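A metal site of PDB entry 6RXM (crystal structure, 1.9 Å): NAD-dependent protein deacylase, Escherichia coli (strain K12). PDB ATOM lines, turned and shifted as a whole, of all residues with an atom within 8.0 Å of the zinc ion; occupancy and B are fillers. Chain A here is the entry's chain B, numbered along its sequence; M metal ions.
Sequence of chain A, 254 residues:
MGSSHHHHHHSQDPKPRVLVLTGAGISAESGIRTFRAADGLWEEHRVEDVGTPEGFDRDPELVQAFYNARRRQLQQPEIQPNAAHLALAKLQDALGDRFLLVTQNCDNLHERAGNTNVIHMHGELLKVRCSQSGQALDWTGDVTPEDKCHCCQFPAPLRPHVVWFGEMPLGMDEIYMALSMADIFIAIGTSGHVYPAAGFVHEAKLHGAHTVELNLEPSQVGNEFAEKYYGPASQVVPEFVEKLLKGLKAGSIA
NE2 of Gln 132 sits close to SG of Cys 149.
The backbone NH (N) of Cys 149 lies within hydrogen-bond range of the backbone carbonyl oxygen (O) of Ala 156.
The side-chain sulfur of Cys 151 sits close to the side-chain hydroxyl of Ser 133, at 3.2 Å.
SG of Cys 130 sits close to NE2 of Gln 132 (3.4 Å).
SG of Cys 130 lies close to N of Ser 133, 3.4 Å away.
N of Cys 130 sits at hydrogen-bond distance from O of Gln 135.
The side-chain sulfur of Cys 152 sits at hydrogen-bond distance from the side-chain amide nitrogen of Gln 132, at 2.5 Å.
The side-chain hydroxyl (OG) of Ser 133 is in hydrogen-bond range of the backbone NH (N) of Gln 135 (3.0 Å).
Ser 133 touches the zinc ion (OG to ZN, 3.99 Å).
Six residues have an atom within 4 Å of the zinc ion: Cys 130, Gln 132, Ser 133, Cys 149, Cys 151 and Cys 152.
Along chain A the residues within 4 Å of the zinc ion span positions 130 to 152.
The zinc ion is bound by the side-chain sulfur (SG) of Cys 149 (2.4 Å).
The zinc ion is bound by the side-chain sulfur (SG) of Cys 151 (2.5 Å).
The zinc ion is bound by the side-chain sulfur (SG) of Cys 130 (2.5 Å).
Slightly farther from the zinc ion lies NE2 of Gln 132 (2.6 Å).
Slightly farther from the zinc ion lies SG of Cys 152 (3.0 Å).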
ATOM      1  N   ARG A 129       7.994  -3.431  15.024  1.00  0.00           N
ATOM      2  CA  ARG A 129       8.453  -2.199  15.611  1.00  0.00           C
ATOM      3  C   ARG A 129       9.936  -2.042  15.395  1.00  0.00           C
ATOM      4  O   ARG A 129      10.730  -2.968  15.562  1.00  0.00           O
ATOM      5  CB  ARG A 129       8.131  -2.166  17.105  1.00  0.00           C
ATOM      6  CG  ARG A 129       8.457  -0.859  17.782  1.00  0.00           C
ATOM      7  CD  ARG A 129       8.452  -1.002  19.303  1.00  0.00           C
ATOM      8  NE  ARG A 129       7.221  -1.626  19.791  1.00  0.00           N
ATOM      9  CZ  ARG A 129       7.062  -2.084  21.037  1.00  0.00           C
ATOM     10  NH1 ARG A 129       8.068  -1.988  21.898  1.00  0.00           N
ATOM     11  NH2 ARG A 129       5.919  -2.627  21.412  1.00  0.00           N
ATOM     12  N   CYS A 130      10.311  -0.835  15.034  1.00  0.00           N
ATOM     13  CA  CYS A 130      11.692  -0.477  14.910  1.00  0.00           C
ATOM     14  C   CYS A 130      12.357  -0.335  16.295  1.00  0.00           C
ATOM     15  O   CYS A 130      11.879   0.409  17.148  1.00  0.00           O
ATOM     16  CB  CYS A 130      11.802   0.820  14.124  1.00  0.00           C
ATOM     17  SG  CYS A 130      13.437   1.474  14.148  1.00  0.00           S
ATOM     18  N   SER A 131      13.453  -1.052  16.502  1.00  0.00           N
ATOM     19  CA  SER A 131      14.139  -1.095  17.799  1.00  0.00           C
ATOM     20  C   SER A 131      14.873   0.199  18.212  1.00  0.00           C
ATOM     21  O   SER A 131      15.422   0.284  19.314  1.00  0.00           O
ATOM     22  CB  SER A 131      15.101  -2.286  17.817  1.00  0.00           C
ATOM     23  OG  SER A 131      16.045  -2.230  16.765  1.00  0.00           O
ATOM     24  N   GLN A 132      14.899   1.200  17.321  1.00  0.00           N
ATOM     25  CA  GLN A 132      15.456   2.524  17.645  1.00  0.00           C
ATOM     26  C   GLN A 132      14.391   3.614  17.707  1.00  0.00           C
ATOM     27  O   GLN A 132      14.303   4.340  18.684  1.00  0.00           O
ATOM     28  CB  GLN A 132      16.535   2.921  16.633  1.00  0.00           C
ATOM     29  CG  GLN A 132      16.156   2.462  15.279  1.00  0.00           C
ATOM     30  CD  GLN A 132      16.852   3.123  14.122  1.00  0.00           C
ATOM     31  OE1 GLN A 132      17.966   3.664  14.237  1.00  0.00           O
ATOM     32  NE2 GLN A 132      16.222   3.020  12.966  1.00  0.00           N
ATOM     33  N   SER A 133      13.570   3.730  16.652  1.00  0.00           N
ATOM     34  CA  SER A 133      12.545   4.768  16.670  1.00  0.00           C
ATOM     35  C   SER A 133      11.341   4.357  17.531  1.00  0.00           C
ATOM     36  O   SER A 133      10.708   5.202  18.152  1.00  0.00           O
ATOM     37  CB  SER A 133      12.082   5.105  15.243  1.00  0.00           C
ATOM     38  OG  SER A 133      11.263   4.094  14.700  1.00  0.00           O
ATOM     39  N   GLY A 134      11.056   3.063  17.584  1.00  0.00           N
ATOM     40  CA  GLY A 134       9.886   2.599  18.285  1.00  0.00           C
ATOM     41  C   GLY A 134       8.635   2.711  17.424  1.00  0.00           C
ATOM     42  O   GLY A 134       7.539   2.421  17.884  1.00  0.00           O
ATOM     43  N   GLN A 135       8.784   3.139  16.178  1.00  0.00           N
ATOM     44  CA  GLN A 135       7.627   3.258  15.290  1.00  0.00           C
ATOM     45  C   GLN A 135       7.168   1.882  14.877  1.00  0.00           C
ATOM     46  O   GLN A 135       7.990   0.985  14.682  1.00  0.00           O
ATOM     47  CB  GLN A 135       7.931   4.087  14.039  1.00  0.00           C
ATOM     48  CG  GLN A 135       7.930   5.599  14.237  1.00  0.00           C
ATOM     49  CD  GLN A 135       8.477   6.346  13.027  1.00  0.00           C
ATOM     50  OE1 GLN A 135       8.374   5.871  11.890  1.00  0.00           O
ATOM     51  NE2 GLN A 135       9.064   7.514  13.263  1.00  0.00           N
ATOM     52  N   LYS A 148      14.815  -5.203   8.124  1.00  0.00           N
ATOM     53  CA  LYS A 148      15.063  -3.972   8.866  1.00  0.00           C
ATOM     54  C   LYS A 148      13.991  -2.921   8.585  1.00  0.00           C
ATOM     55  O   LYS A 148      13.126  -3.098   7.726  1.00  0.00           O
ATOM     56  CB  LYS A 148      16.434  -3.366   8.567  1.00  0.00           C
ATOM     57  CG  LYS A 148      17.566  -3.889   9.427  1.00  0.00           C
ATOM     58  CD  LYS A 148      18.271  -5.072   8.844  1.00  0.00           C
ATOM     59  CE  LYS A 148      18.941  -5.839   9.960  1.00  0.00           C
ATOM     60  NZ  LYS A 148      19.225  -7.220   9.545  1.00  0.00           N
ATOM     61  N   CYS A 149      14.068  -1.841   9.346  1.00  0.00           N
ATOM     62  CA  CYS A 149      13.042  -0.806   9.378  1.00  0.00           C
ATOM     63  C   CYS A 149      12.920   0.028   8.098  1.00  0.00           C
ATOM     64  O   CYS A 149      13.767  -0.052   7.198  1.00  0.00           O
ATOM     65  CB  CYS A 149      13.318   0.135  10.547  1.00  0.00           C
ATOM     66  SG  CYS A 149      14.649   1.288  10.214  1.00  0.00           S
ATOM     67  N   HIS A 150      11.854   0.822   8.033  1.00  0.00           N
ATOM     68  CA  HIS A 150      11.610   1.706   6.905  1.00  0.00           C
ATOM     69  C   HIS A 150      11.534   3.161   7.361  1.00  0.00           C
ATOM     70  O   HIS A 150      11.053   4.014   6.612  1.00  0.00           O
ATOM     71  CB  HIS A 150      10.282   1.396   6.210  1.00  0.00           C
ATOM     72  CG  HIS A 150      10.086  -0.046   5.864  1.00  0.00           C
ATOM     73  ND1 HIS A 150       8.839  -0.560   5.562  1.00  0.00           N
ATOM     74  CD2 HIS A 150      10.947  -1.087   5.795  1.00  0.00           C
ATOM     75  CE1 HIS A 150       8.949  -1.856   5.294  1.00  0.00           C
ATOM     76  NE2 HIS A 150      10.213  -2.200   5.434  1.00  0.00           N
ATOM     77  N   CYS A 151      11.978   3.442   8.581  1.00  0.00           N
ATOM     78  CA  CYS A 151      11.827   4.783   9.144  1.00  0.00           C
ATOM     79  C   CYS A 151      13.127   5.541   9.415  1.00  0.00           C
ATOM     80  O   CYS A 151      13.094   6.729   9.761  1.00  0.00           O
ATOM     81  CB  CYS A 151      10.983   4.710  10.433  1.00  0.00           C
ATOM     82  SG  CYS A 151      11.478   3.428  11.615  1.00  0.00           S
ATOM     83  N   CYS A 152      14.267   4.874   9.325  1.00  0.00           N
ATOM     84  CA  CYS A 152      15.544   5.562   9.499  1.00  0.00           C
ATOM     85  C   CYS A 152      16.438   5.326   8.289  1.00  0.00           C
ATOM     86  O   CYS A 152      16.299   4.315   7.602  1.00  0.00           O
ATOM     87  CB  CYS A 152      16.243   5.131  10.797  1.00  0.00           C
ATOM     88  SG  CYS A 152      15.252   5.285  12.323  1.00  0.00           S
ATOM     89  N   GLN A 153      17.377   6.250   8.077  1.00  0.00           N
ATOM     90  CA  GLN A 153      18.283   6.145   6.945  1.00  0.00           C
ATOM     91  C   GLN A 153      19.220   4.957   7.106  1.00  0.00           C
ATOM     92  O   GLN A 153      19.596   4.302   6.118  1.00  0.00           O
ATOM     93  CB  GLN A 153      19.103   7.433   6.756  1.00  0.00           C
ATOM     94  CG  GLN A 153      18.361   8.388   5.846  1.00  0.00           C
ATOM     95  CD  GLN A 153      18.488   7.980   4.395  1.00  0.00           C
ATOM     96  OE1 GLN A 153      19.553   8.090   3.771  1.00  0.00           O
ATOM     97  NE2 GLN A 153      17.408   7.429   3.867  1.00  0.00           N
ATOM     98  N   PHE A 154      19.594   4.665   8.353  1.00  0.00           N
ATOM     99  CA  PHE A 154      20.363   3.470   8.628  1.00  0.00           C
ATOM    100  C   PHE A 154      19.464   2.480   9.359  1.00  0.00           C
ATOM    101  O   PHE A 154      19.189   2.647  10.558  1.00  0.00           O
ATOM    102  CB  PHE A 154      21.616   3.783   9.448  1.00  0.00           C
ATOM    103  CG  PHE A 154      22.141   2.603  10.219  1.00  0.00           C
ATOM    104  CD1 PHE A 154      22.772   1.561   9.564  1.00  0.00           C
ATOM    105  CD2 PHE A 154      22.058   2.558  11.609  1.00  0.00           C
ATOM    106  CE1 PHE A 154      23.266   0.469  10.264  1.00  0.00           C
ATOM    107  CE2 PHE A 154      22.557   1.474  12.311  1.00  0.00           C
ATOM    108  CZ  PHE A 154      23.161   0.428  11.646  1.00  0.00           C
ATOM    109  N   PRO A 155      19.000   1.461   8.628  1.00  0.00           N
ATOM    110  CA  PRO A 155      18.025   0.430   9.010  1.00  0.00           C
ATOM    111  C   PRO A 155      18.384  -0.347  10.279  1.00  0.00           C
ATOM    112  O   PRO A 155      19.495  -0.862  10.377  1.00  0.00           O
ATOM    113  CB  PRO A 155      18.021  -0.504   7.793  1.00  0.00           C
ATOM    114  CG  PRO A 155      18.483   0.317   6.649  1.00  0.00           C
ATOM    115  CD  PRO A 155      19.410   1.336   7.217  1.00  0.00           C
ATOM    116  N   ALA A 156      17.446  -0.426  11.217  1.00  0.00           N
ATOM    117  CA  ALA A 156      17.690  -1.095  12.498  1.00  0.00           C
ATOM    118  C   ALA A 156      16.963  -2.427  12.578  1.00  0.00           C
ATOM    119  O   ALA A 156      15.995  -2.643  11.847  1.00  0.00           O
ATOM    120  CB  ALA A 156      17.280  -0.199  13.628  1.00  0.00           C
ATOM    121  N   PRO A 157      17.428  -3.340  13.458  1.00  0.00           N
ATOM    122  CA  PRO A 157      16.709  -4.611  13.609  1.00  0.00           C
ATOM    123  C   PRO A 157      15.256  -4.395  14.050  1.00  0.00           C
ATOM    124  O   PRO A 157      14.942  -3.424  14.754  1.00  0.00           O
ATOM    125  CB  PRO A 157      17.528  -5.364  14.677  1.00  0.00           C
ATOM    126  CG  PRO A 157      18.320  -4.303  15.372  1.00  0.00           C
ATOM    127  CD  PRO A 157      18.602  -3.260  14.338  1.00  0.00           C
ATOM    128  N   LEU A 158      14.386  -5.296  13.635  1.00  0.00           N
ATOM    129  CA  LEU A 158      12.975  -5.205  13.987  1.00  0.00           C
ATOM    130  C   LEU A 158      12.610  -6.148  15.122  1.00  0.00           C
ATOM    131  O   LEU A 158      13.179  -7.239  15.220  1.00  0.00           O
ATOM    132  CB  LEU A 158      12.102  -5.514  12.774  1.00  0.00           C
ATOM    133  CG  LEU A 158      12.180  -4.544  11.591  1.00  0.00           C
ATOM    134  CD1 LEU A 158      11.470  -5.139  10.412  1.00  0.00           C
ATOM    135  CD2 LEU A 158      11.564  -3.206  11.968  1.00  0.00           C
HETATM  136 ZN    ZN M   1      13.809   2.688  11.969  1.00  0.00          ZN
